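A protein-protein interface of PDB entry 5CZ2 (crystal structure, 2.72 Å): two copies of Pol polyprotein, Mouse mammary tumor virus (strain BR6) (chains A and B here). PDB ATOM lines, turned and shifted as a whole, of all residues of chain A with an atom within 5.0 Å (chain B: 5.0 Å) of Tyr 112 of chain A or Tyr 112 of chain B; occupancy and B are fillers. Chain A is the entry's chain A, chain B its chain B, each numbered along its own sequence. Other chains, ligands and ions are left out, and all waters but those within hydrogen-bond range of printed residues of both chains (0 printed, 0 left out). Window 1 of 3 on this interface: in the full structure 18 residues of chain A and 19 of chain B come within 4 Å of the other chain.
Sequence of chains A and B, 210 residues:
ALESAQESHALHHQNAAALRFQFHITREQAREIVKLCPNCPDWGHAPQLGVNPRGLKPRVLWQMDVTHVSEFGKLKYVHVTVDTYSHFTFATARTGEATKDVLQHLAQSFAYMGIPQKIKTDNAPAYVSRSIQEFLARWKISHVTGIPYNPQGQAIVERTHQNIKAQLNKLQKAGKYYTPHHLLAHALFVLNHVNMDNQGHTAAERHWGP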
ATOM      1  N   PHE A  88      -6.524  14.316   7.193  1.00  0.00           N
ATOM      2  CA  PHE A  88      -7.809  14.558   7.831  1.00  0.00           C
ATOM      3  C   PHE A  88      -8.247  13.300   8.571  1.00  0.00           C
ATOM      4  O   PHE A  88      -8.302  12.212   7.993  1.00  0.00           O
ATOM      5  CB  PHE A  88      -8.843  14.962   6.778  1.00  0.00           C
ATOM      6  CG  PHE A  88     -10.050  15.655   7.340  1.00  0.00           C
ATOM      7  CD1 PHE A  88     -11.316  15.129   7.152  1.00  0.00           C
ATOM      8  CD2 PHE A  88      -9.922  16.840   8.045  1.00  0.00           C
ATOM      9  CE1 PHE A  88     -12.430  15.766   7.660  1.00  0.00           C
ATOM     10  CE2 PHE A  88     -11.032  17.481   8.559  1.00  0.00           C
ATOM     11  CZ  PHE A  88     -12.286  16.944   8.366  1.00  0.00           C
ATOM     12  N   THR A  89      -8.555  13.451   9.857  1.00  0.00           N
ATOM     13  CA  THR A  89      -8.725  12.321  10.761  1.00  0.00           C
ATOM     14  C   THR A  89     -10.119  12.337  11.374  1.00  0.00           C
ATOM     15  O   THR A  89     -10.596  13.386  11.817  1.00  0.00           O
ATOM     16  CB  THR A  89      -7.661  12.347  11.866  1.00  0.00           C
ATOM     17  OG1 THR A  89      -6.390  11.982  11.315  1.00  0.00           O
ATOM     18  CG2 THR A  89      -8.019  11.384  12.989  1.00  0.00           C
ATOM     19  N   PHE A  90     -10.759  11.171  11.397  1.00  0.00           N
ATOM     20  CA  PHE A  90     -12.027  10.971  12.082  1.00  0.00           C
ATOM     21  C   PHE A  90     -11.898   9.787  13.030  1.00  0.00           C
ATOM     22  O   PHE A  90     -11.184   8.821  12.744  1.00  0.00           O
ATOM     23  CB  PHE A  90     -13.168  10.731  11.086  1.00  0.00           C
ATOM     24  CG  PHE A  90     -14.487  10.441  11.737  1.00  0.00           C
ATOM     25  CD1 PHE A  90     -15.050   9.179  11.659  1.00  0.00           C
ATOM     26  CD2 PHE A  90     -15.155  11.427  12.441  1.00  0.00           C
ATOM     27  CE1 PHE A  90     -16.262   8.912  12.261  1.00  0.00           C
ATOM     28  CE2 PHE A  90     -16.367  11.166  13.045  1.00  0.00           C
ATOM     29  CZ  PHE A  90     -16.921   9.909  12.954  1.00  0.00           C
ATOM     30  N   GLN A 108     -20.278   6.992   9.739  1.00  0.00           N
ATOM     31  CA  GLN A 108     -19.905   8.259  10.359  1.00  0.00           C
ATOM     32  C   GLN A 108     -18.708   8.890   9.657  1.00  0.00           C
ATOM     33  O   GLN A 108     -18.653  10.116   9.492  1.00  0.00           O
ATOM     34  CB  GLN A 108     -19.609   8.049  11.842  1.00  0.00           C
ATOM     35  CG  GLN A 108     -20.809   7.619  12.666  1.00  0.00           C
ATOM     36  CD  GLN A 108     -21.102   8.575  13.805  1.00  0.00           C
ATOM     37  OE1 GLN A 108     -20.688   8.350  14.942  1.00  0.00           O
ATOM     38  NE2 GLN A 108     -21.819   9.653  13.504  1.00  0.00           N
ATOM     39  N   SER A 109     -17.734   8.071   9.250  1.00  0.00           N
ATOM     40  CA  SER A 109     -16.597   8.579   8.486  1.00  0.00           C
ATOM     41  C   SER A 109     -17.051   9.260   7.201  1.00  0.00           C
ATOM     42  O   SER A 109     -16.503  10.299   6.813  1.00  0.00           O
ATOM     43  CB  SER A 109     -15.623   7.444   8.175  1.00  0.00           C
ATOM     44  OG  SER A 109     -15.116   6.862   9.363  1.00  0.00           O
ATOM     45  N   PHE A 110     -18.046   8.684   6.522  1.00  0.00           N
ATOM     46  CA  PHE A 110     -18.469   9.214   5.231  1.00  0.00           C
ATOM     47  C   PHE A 110     -19.143  10.572   5.381  1.00  0.00           C
ATOM     48  O   PHE A 110     -18.904  11.481   4.577  1.00  0.00           O
ATOM     49  CB  PHE A 110     -19.404   8.221   4.540  1.00  0.00           C
ATOM     50  CG  PHE A 110     -18.758   6.902   4.219  1.00  0.00           C
ATOM     51  CD1 PHE A 110     -17.380   6.793   4.120  1.00  0.00           C
ATOM     52  CD2 PHE A 110     -19.530   5.768   4.023  1.00  0.00           C
ATOM     53  CE1 PHE A 110     -16.786   5.581   3.828  1.00  0.00           C
ATOM     54  CE2 PHE A 110     -18.941   4.554   3.732  1.00  0.00           C
ATOM     55  CZ  PHE A 110     -17.567   4.460   3.635  1.00  0.00           C
ATOM     56  N   ALA A 111     -19.997  10.727   6.395  1.00  0.00           N
ATOM     57  CA  ALA A 111     -20.585  12.033   6.670  1.00  0.00           C
ATOM     58  C   ALA A 111     -19.524  13.049   7.071  1.00  0.00           C
ATOM     59  O   ALA A 111     -19.656  14.240   6.765  1.00  0.00           O
ATOM     60  CB  ALA A 111     -21.646  11.913   7.763  1.00  0.00           C
ATOM     61  N   TYR A 112     -18.469  12.599   7.751  1.00  0.00           N
ATOM     62  CA  TYR A 112     -17.439  13.506   8.244  1.00  0.00           C
ATOM     63  C   TYR A 112     -16.434  13.876   7.158  1.00  0.00           C
ATOM     64  O   TYR A 112     -15.975  15.022   7.102  1.00  0.00           O
ATOM     65  CB  TYR A 112     -16.725  12.872   9.437  1.00  0.00           C
ATOM     66  CG  TYR A 112     -15.869  13.822  10.244  1.00  0.00           C
ATOM     67  CD1 TYR A 112     -16.408  14.548  11.297  1.00  0.00           C
ATOM     68  CD2 TYR A 112     -14.517  13.978   9.964  1.00  0.00           C
ATOM     69  CE1 TYR A 112     -15.627  15.412  12.042  1.00  0.00           C
ATOM     70  CE2 TYR A 112     -13.729  14.839  10.703  1.00  0.00           C
ATOM     71  CZ  TYR A 112     -14.288  15.553  11.740  1.00  0.00           C
ATOM     72  OH  TYR A 112     -13.508  16.411  12.479  1.00  0.00           O
ATOM     73  N   MET A 113     -16.078  12.927   6.290  1.00  0.00           N
ATOM     74  CA  MET A 113     -14.961  13.111   5.373  1.00  0.00           C
ATOM     75  C   MET A 113     -15.297  12.910   3.903  1.00  0.00           C
ATOM     76  O   MET A 113     -14.470  13.260   3.053  1.00  0.00           O
ATOM     77  CB  MET A 113     -13.815  12.155   5.734  1.00  0.00           C
ATOM     78  CG  MET A 113     -13.312  12.272   7.158  1.00  0.00           C
ATOM     79  SD  MET A 113     -12.118  10.979   7.552  1.00  0.00           S
ATOM     80  CE  MET A 113     -10.871  11.291   6.305  1.00  0.00           C
ATOM     81  N   GLY A 114     -16.461  12.372   3.570  1.00  0.00           N
ATOM     82  CA  GLY A 114     -16.780  12.037   2.198  1.00  0.00           C
ATOM     83  C   GLY A 114     -16.525  10.576   1.889  1.00  0.00           C
ATOM     84  O   GLY A 114     -16.379   9.733   2.777  1.00  0.00           O
ATOM     85  N   LEU A 188     -10.606  15.861  18.101  1.00  0.00           N
ATOM     86  CA  LEU A 188     -10.695  15.872  16.643  1.00  0.00           C
ATOM     87  C   LEU A 188     -10.761  17.294  16.102  1.00  0.00           C
ATOM     88  O   LEU A 188     -10.160  17.601  15.064  1.00  0.00           O
ATOM     89  CB  LEU A 188     -11.911  15.069  16.184  1.00  0.00           C
ATOM     90  CG  LEU A 188     -11.869  13.561  16.439  1.00  0.00           C
ATOM     91  CD1 LEU A 188     -13.206  12.921  16.097  1.00  0.00           C
ATOM     92  CD2 LEU A 188     -10.741  12.914  15.652  1.00  0.00           C
ATOM     93  N   ASN A 192      -7.874  18.659  13.410  1.00  0.00           N
ATOM     94  CA  ASN A 192      -8.325  18.879  12.041  1.00  0.00           C
ATOM     95  C   ASN A 192      -8.539  20.350  11.710  1.00  0.00           C
ATOM     96  O   ASN A 192      -8.231  20.778  10.592  1.00  0.00           O
ATOM     97  CB  ASN A 192      -9.622  18.108  11.788  1.00  0.00           C
ATOM     98  CG  ASN A 192      -9.416  16.609  11.791  1.00  0.00           C
ATOM     99  OD1 ASN A 192      -8.355  16.116  11.408  1.00  0.00           O
ATOM    100  ND2 ASN A 192     -10.432  15.873  12.228  1.00  0.00           N
ATOM    101  N   HIS A 193      -9.058  21.136  12.649  1.00  0.00           N
ATOM    102  CA  HIS A 193      -9.492  22.495  12.359  1.00  0.00           C
ATOM    103  C   HIS A 193      -8.660  23.567  13.049  1.00  0.00           C
ATOM    104  O   HIS A 193      -8.925  24.757  12.845  1.00  0.00           O
ATOM    105  CB  HIS A 193     -10.965  22.661  12.743  1.00  0.00           C
ATOM    106  CG  HIS A 193     -11.870  21.654  12.104  1.00  0.00           C
ATOM    107  ND1 HIS A 193     -12.402  21.825  10.844  1.00  0.00           N
ATOM    108  CD2 HIS A 193     -12.332  20.461  12.550  1.00  0.00           C
ATOM    109  CE1 HIS A 193     -13.156  20.781  10.543  1.00  0.00           C
ATOM    110  NE2 HIS A 193     -13.129  19.940  11.561  1.00  0.00           N
ATOM    111  N   TRP A 208     -10.252  19.735   1.744  1.00  0.00           N
ATOM    112  CA  TRP A 208     -11.254  20.371   0.892  1.00  0.00           C
ATOM    113  C   TRP A 208     -10.632  21.584   0.195  1.00  0.00           C
ATOM    114  O   TRP A 208     -11.121  22.710   0.295  1.00  0.00           O
ATOM    115  CB  TRP A 208     -12.487  20.793   1.691  1.00  0.00           C
ATOM    116  CG  TRP A 208     -13.036  19.744   2.609  1.00  0.00           C
ATOM    117  CD1 TRP A 208     -12.826  19.643   3.953  1.00  0.00           C
ATOM    118  CD2 TRP A 208     -13.908  18.662   2.256  1.00  0.00           C
ATOM    119  NE1 TRP A 208     -13.501  18.558   4.458  1.00  0.00           N
ATOM    120  CE2 TRP A 208     -14.173  17.939   3.436  1.00  0.00           C
ATOM    121  CE3 TRP A 208     -14.484  18.231   1.057  1.00  0.00           C
ATOM    122  CZ2 TRP A 208     -14.989  16.811   3.452  1.00  0.00           C
ATOM    123  CZ3 TRP A 208     -15.294  17.109   1.075  1.00  0.00           C
ATOM    124  CH2 TRP A 208     -15.539  16.412   2.265  1.00  0.00           C
ATOM    125  N   PHE B  88     -24.117  23.998   5.277  1.00  0.00           N
ATOM    126  CA  PHE B  88     -23.493  22.798   5.815  1.00  0.00           C
ATOM    127  C   PHE B  88     -24.185  22.410   7.115  1.00  0.00           C
ATOM    128  O   PHE B  88     -24.303  23.224   8.035  1.00  0.00           O
ATOM    129  CB  PHE B  88     -22.000  23.045   6.038  1.00  0.00           C
ATOM    130  CG  PHE B  88     -21.181  21.791   6.157  1.00  0.00           C
ATOM    131  CD1 PHE B  88     -20.454  21.528   7.305  1.00  0.00           C
ATOM    132  CD2 PHE B  88     -21.132  20.878   5.118  1.00  0.00           C
ATOM    133  CE1 PHE B  88     -19.696  20.381   7.417  1.00  0.00           C
ATOM    134  CE2 PHE B  88     -20.376  19.725   5.224  1.00  0.00           C
ATOM    135  CZ  PHE B  88     -19.658  19.476   6.374  1.00  0.00           C
ATOM    136  N   THR B  89     -24.648  21.165   7.190  1.00  0.00           N
ATOM    137  CA  THR B  89     -25.552  20.726   8.245  1.00  0.00           C
ATOM    138  C   THR B  89     -24.945  19.564   9.018  1.00  0.00           C
ATOM    139  O   THR B  89     -24.419  18.620   8.420  1.00  0.00           O
ATOM    140  CB  THR B  89     -26.909  20.314   7.659  1.00  0.00           C
ATOM    141  OG1 THR B  89     -27.628  21.482   7.246  1.00  0.00           O
ATOM    142  CG2 THR B  89     -27.735  19.549   8.684  1.00  0.00           C
ATOM    143  N   PHE B  90     -25.021  19.642  10.346  1.00  0.00           N
ATOM    144  CA  PHE B  90     -24.640  18.554  11.232  1.00  0.00           C
ATOM    145  C   PHE B  90     -25.791  18.271  12.186  1.00  0.00           C
ATOM    146  O   PHE B  90     -26.497  19.193  12.606  1.00  0.00           O
ATOM    147  CB  PHE B  90     -23.369  18.892  12.014  1.00  0.00           C
ATOM    148  CG  PHE B  90     -22.970  17.840  13.004  1.00  0.00           C
ATOM    149  CD1 PHE B  90     -23.054  18.082  14.365  1.00  0.00           C
ATOM    150  CD2 PHE B  90     -22.522  16.603  12.575  1.00  0.00           C
ATOM    151  CE1 PHE B  90     -22.689  17.114  15.276  1.00  0.00           C
ATOM    152  CE2 PHE B  90     -22.154  15.630  13.481  1.00  0.00           C
ATOM    153  CZ  PHE B  90     -22.237  15.885  14.832  1.00  0.00           C
ATOM    154  N   GLN B 108     -19.394  18.035  19.119  1.00  0.00           N
ATOM    155  CA  GLN B 108     -19.418  17.287  17.866  1.00  0.00           C
ATOM    156  C   GLN B 108     -19.572  18.219  16.671  1.00  0.00           C
ATOM    157  O   GLN B 108     -18.967  17.990  15.617  1.00  0.00           O
ATOM    158  CB  GLN B 108     -20.541  16.251  17.894  1.00  0.00           C
ATOM    159  CG  GLN B 108     -20.422  15.237  19.017  1.00  0.00           C
ATOM    160  CD  GLN B 108     -20.577  13.812  18.531  1.00  0.00           C
ATOM    161  OE1 GLN B 108     -21.655  13.225  18.623  1.00  0.00           O
ATOM    162  NE2 GLN B 108     -19.496  13.245  18.009  1.00  0.00           N
ATOM    163  N   SER B 109     -20.392  19.265  16.812  1.00  0.00           N
ATOM    164  CA  SER B 109     -20.532  20.256  15.748  1.00  0.00           C
ATOM    165  C   SER B 109     -19.194  20.896  15.400  1.00  0.00           C
ATOM    166  O   SER B 109     -18.896  21.123  14.221  1.00  0.00           O
ATOM    167  CB  SER B 109     -21.545  21.324  16.158  1.00  0.00           C
ATOM    168  OG  SER B 109     -22.822  20.756  16.390  1.00  0.00           O
ATOM    169  N   PHE B 110     -18.375  21.197  16.411  1.00  0.00           N
ATOM    170  CA  PHE B 110     -17.120  21.901  16.160  1.00  0.00           C
ATOM    171  C   PHE B 110     -16.131  21.023  15.405  1.00  0.00           C
ATOM    172  O   PHE B 110     -15.447  21.496  14.489  1.00  0.00           O
ATOM    173  CB  PHE B 110     -16.513  22.384  17.478  1.00  0.00           C
ATOM    174  CG  PHE B 110     -17.360  23.389  18.205  1.00  0.00           C
ATOM    175  CD1 PHE B 110     -18.316  24.130  17.530  1.00  0.00           C
ATOM    176  CD2 PHE B 110     -17.195  23.599  19.564  1.00  0.00           C
ATOM    177  CE1 PHE B 110     -19.094  25.055  18.196  1.00  0.00           C
ATOM    178  CE2 PHE B 110     -17.969  24.524  20.238  1.00  0.00           C
ATOM    179  CZ  PHE B 110     -18.921  25.253  19.552  1.00  0.00           C
ATOM    180  N   ALA B 111     -16.030  19.747  15.780  1.00  0.00           N
ATOM    181  CA  ALA B 111     -15.191  18.821  15.025  1.00  0.00           C
ATOM    182  C   ALA B 111     -15.703  18.636  13.602  1.00  0.00           C
ATOM    183  O   ALA B 111     -14.910  18.429  12.677  1.00  0.00           O
ATOM    184  CB  ALA B 111     -15.113  17.474  15.743  1.00  0.00           C
ATOM    185  N   TYR B 112     -17.020  18.709  13.411  1.00  0.00           N
ATOM    186  CA  TYR B 112     -17.613  18.465  12.101  1.00  0.00           C
ATOM    187  C   TYR B 112     -17.525  19.692  11.199  1.00  0.00           C
ATOM    188  O   TYR B 112     -17.298  19.559   9.991  1.00  0.00           O
ATOM    189  CB  TYR B 112     -19.070  18.031  12.275  1.00  0.00           C
ATOM    190  CG  TYR B 112     -19.712  17.422  11.049  1.00  0.00           C
ATOM    191  CD1 TYR B 112     -19.625  16.058  10.804  1.00  0.00           C
ATOM    192  CD2 TYR B 112     -20.426  18.204  10.151  1.00  0.00           C
ATOM    193  CE1 TYR B 112     -20.220  15.492   9.693  1.00  0.00           C
ATOM    194  CE2 TYR B 112     -21.025  17.647   9.036  1.00  0.00           C
ATOM    195  CZ  TYR B 112     -20.917  16.292   8.812  1.00  0.00           C
ATOM    196  OH  TYR B 112     -21.511  15.732   7.705  1.00  0.00           O
ATOM    197  N   MET B 113     -17.695  20.889  11.763  1.00  0.00           N
ATOM    198  CA  MET B 113     -17.860  22.095  10.962  1.00  0.00           C
ATOM    199  C   MET B 113     -16.878  23.215  11.277  1.00  0.00           C
ATOM    200  O   MET B 113     -16.807  24.174  10.501  1.00  0.00           O
ATOM    201  CB  MET B 113     -19.283  22.649  11.124  1.00  0.00           C
ATOM    202  CG  MET B 113     -20.389  21.673  10.784  1.00  0.00           C
ATOM    203  SD  MET B 113     -22.007  22.343  11.207  1.00  0.00           S
ATOM    204  CE  MET B 113     -22.015  23.843  10.229  1.00  0.00           C
ATOM    205  N   GLY B 114     -16.125  23.134  12.365  1.00  0.00           N
ATOM    206  CA  GLY B 114     -15.272  24.229  12.784  1.00  0.00           C
ATOM    207  C   GLY B 114     -15.917  25.096  13.846  1.00  0.00           C
ATOM    208  O   GLY B 114     -16.886  24.714  14.506  1.00  0.00           O
ATOM    209  N   LEU B 188     -26.833  12.659   6.524  1.00  0.00           N
ATOM    210  CA  LEU B 188     -25.910  13.790   6.541  1.00  0.00           C
ATOM    211  C   LEU B 188     -24.906  13.703   5.397  1.00  0.00           C
ATOM    212  O   LEU B 188     -24.562  14.721   4.786  1.00  0.00           O
ATOM    213  CB  LEU B 188     -25.181  13.858   7.883  1.00  0.00           C
ATOM    214  CG  LEU B 188     -26.026  14.199   9.109  1.00  0.00           C
ATOM    215  CD1 LEU B 188     -25.201  14.047  10.374  1.00  0.00           C
ATOM    216  CD2 LEU B 188     -26.577  15.609   8.992  1.00  0.00           C
ATOM    217  N   ASN B 192     -24.769  16.756   2.622  1.00  0.00           N
ATOM    218  CA  ASN B 192     -23.581  17.600   2.667  1.00  0.00           C
ATOM    219  C   ASN B 192     -22.579  17.285   1.562  1.00  0.00           C
ATOM    220  O   ASN B 192     -21.953  18.203   1.023  1.00  0.00           O
ATOM    221  CB  ASN B 192     -22.896  17.468   4.031  1.00  0.00           C
ATOM    222  CG  ASN B 192     -23.718  18.064   5.156  1.00  0.00           C
ATOM    223  OD1 ASN B 192     -24.451  19.033   4.959  1.00  0.00           O
ATOM    224  ND2 ASN B 192     -23.599  17.486   6.345  1.00  0.00           N
ATOM    225  N   HIS B 193     -22.407  16.011   1.216  1.00  0.00           N
ATOM    226  CA  HIS B 193     -21.333  15.596   0.327  1.00  0.00           C
ATOM    227  C   HIS B 193     -21.813  15.064  -1.017  1.00  0.00           C
ATOM    228  O   HIS B 193     -20.977  14.715  -1.857  1.00  0.00           O
ATOM    229  CB  HIS B 193     -20.467  14.535   1.016  1.00  0.00           C
ATOM    230  CG  HIS B 193     -19.928  14.966   2.344  1.00  0.00           C
ATOM    231  ND1 HIS B 193     -18.764  15.691   2.475  1.00  0.00           N
ATOM    232  CD2 HIS B 193     -20.398  14.779   3.600  1.00  0.00           C
ATOM    233  CE1 HIS B 193     -18.538  15.930   3.756  1.00  0.00           C
ATOM    234  NE2 HIS B 193     -19.515  15.388   4.459  1.00  0.00           N
ATOM    235  N   TRP B 208     -15.965  24.972   2.745  1.00  0.00           N
ATOM    236  CA  TRP B 208     -14.506  25.025   2.744  1.00  0.00           C
ATOM    237  C   TRP B 208     -13.995  25.494   1.388  1.00  0.00           C
ATOM    238  O   TRP B 208     -13.085  24.908   0.797  1.00  0.00           O
ATOM    239  CB  TRP B 208     -13.912  23.664   3.095  1.00  0.00           C
ATOM    240  CG  TRP B 208     -14.528  23.021   4.295  1.00  0.00           C
ATOM    241  CD1 TRP B 208     -15.486  22.049   4.302  1.00  0.00           C
ATOM    242  CD2 TRP B 208     -14.220  23.290   5.668  1.00  0.00           C
ATOM    243  NE1 TRP B 208     -15.801  21.702   5.593  1.00  0.00           N
ATOM    244  CE2 TRP B 208     -15.037  22.448   6.450  1.00  0.00           C
ATOM    245  CE3 TRP B 208     -13.336  24.162   6.309  1.00  0.00           C
ATOM    246  CZ2 TRP B 208     -14.994  22.454   7.843  1.00  0.00           C
ATOM    247  CZ3 TRP B 208     -13.296  24.166   7.692  1.00  0.00           C
ATOM    248  CH2 TRP B 208     -14.121  23.318   8.443  1.00  0.00           C
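Phe 110 of chain A touches His 193 of chain B, and with the chains exchanged His 193 of chain A touches Phe 110 of chain B. Ala 111 of chain A touches Tyr 112 of chain B, and with the chains exchanged Tyr 112 of chain A touches Ala 111 of chain B. Ala 111 of chain A touches His 193 of chain B, and with the chains exchanged His 193 of chain A touches Ala 111 of chain B. Trp 208 of chain A touches its own counterpart, Trp 208 of chain B. Positions printed for both chains: 88, 89, 90, 108, 109, 110, 111, 112, 113, 114, 188, 192, 193 and 208.
Among the printed residues, merely in contact across the chains: His 193 of chain A with Trp 208 of chain B (3.3 Å), Trp 208 of chain A with His 193 of chain B (3.3 Å), Tyr 112 of chain A with Tyr 112 of chain B (3.6 Å), Phe 110 of chain A with His 193 of chain B (3.8 Å) and His 193 of chain A with Phe 110 of chain B (3.8 Å).
Of the 14 printed residues of chain A, 5 touch a printed residue of chain B. Printed residues of chain A that touch a printed residue of chain B: Phe 110, Ala 111, Tyr 112, His 193 and Trp 208. Of the 14 printed residues of chain B, 5 touch a printed residue of chain A. Hydrophobic or aromatic side chains of chain B within 4 Å of the printed part of chain A: Ala 111, Tyr 112, His 193 and Trp 208.
The side-chain amide nitrogen (ND2) of Asn 192 of chain A sits at hydrogen-bond distance from the side-chain hydroxyl (OH) of Tyr 112 of chain A (3.1 Å). The side-chain amide nitrogen of Asn 192 of chain B sits at hydrogen-bond distance from the side-chain hydroxyl of Tyr 112 of chain B.
Ser 109 of chain A touches none of the printed residues of chain B. Of the printed residues of chain B, Ala 111 of chain A touches Tyr 112 (2.6 Å) and His 193 (2.6 Å). Of the printed residues of chain B, Tyr 112 of chain A touches Ala 111 and Tyr 112. Of the printed residues of chain B, His 193 of chain A touches Phe 110 (3.8 Å), Ala 111 (2.6 Å) and Trp 208 (3.3 Å). Printed residues of chain A within 4 Å of Phe 110 of chain B: His 193 (3.8 Å). Printed residues of chain A within 4 Å of Ala 111 of chain B: Tyr 112 (2.5 Å) and His 193 (2.6 Å). Tyr 112 of chain B touches just these residues of chain A: Ala 111 and Tyr 112. Of the printed residues of chain A, His 193 of chain B touches Phe 110, Ala 111 and Trp 208. The nearest residue of chain A that does not touch Tyr 112 of chain B is His 193 of chain A (4.4 Å).
The backbone carbonyl oxygen (O) of Ala 111 of chain A lies within hydrogen-bond range of the side-chain hydroxyl (OH) of Tyr 112 of chain B. NE2 of His 193 of chain B sits at hydrogen-bond distance from O of Ala 111 of chain A. OH of Tyr 112 of chain A is in hydrogen-bond range of O of Ala 111 of chain B, at 2.5 Å. A ring nitrogen (NE2) of His 193 of chain A is in hydrogen-bond range of the backbone carbonyl oxygen (O) of Ala 111 of chain B (2.6 Å). The backbone carbonyl oxygen (O) of Trp 208 of chain A lies close to the backbone carbonyl oxygen (O) of Trp 208 of chain B (3.0 Å).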
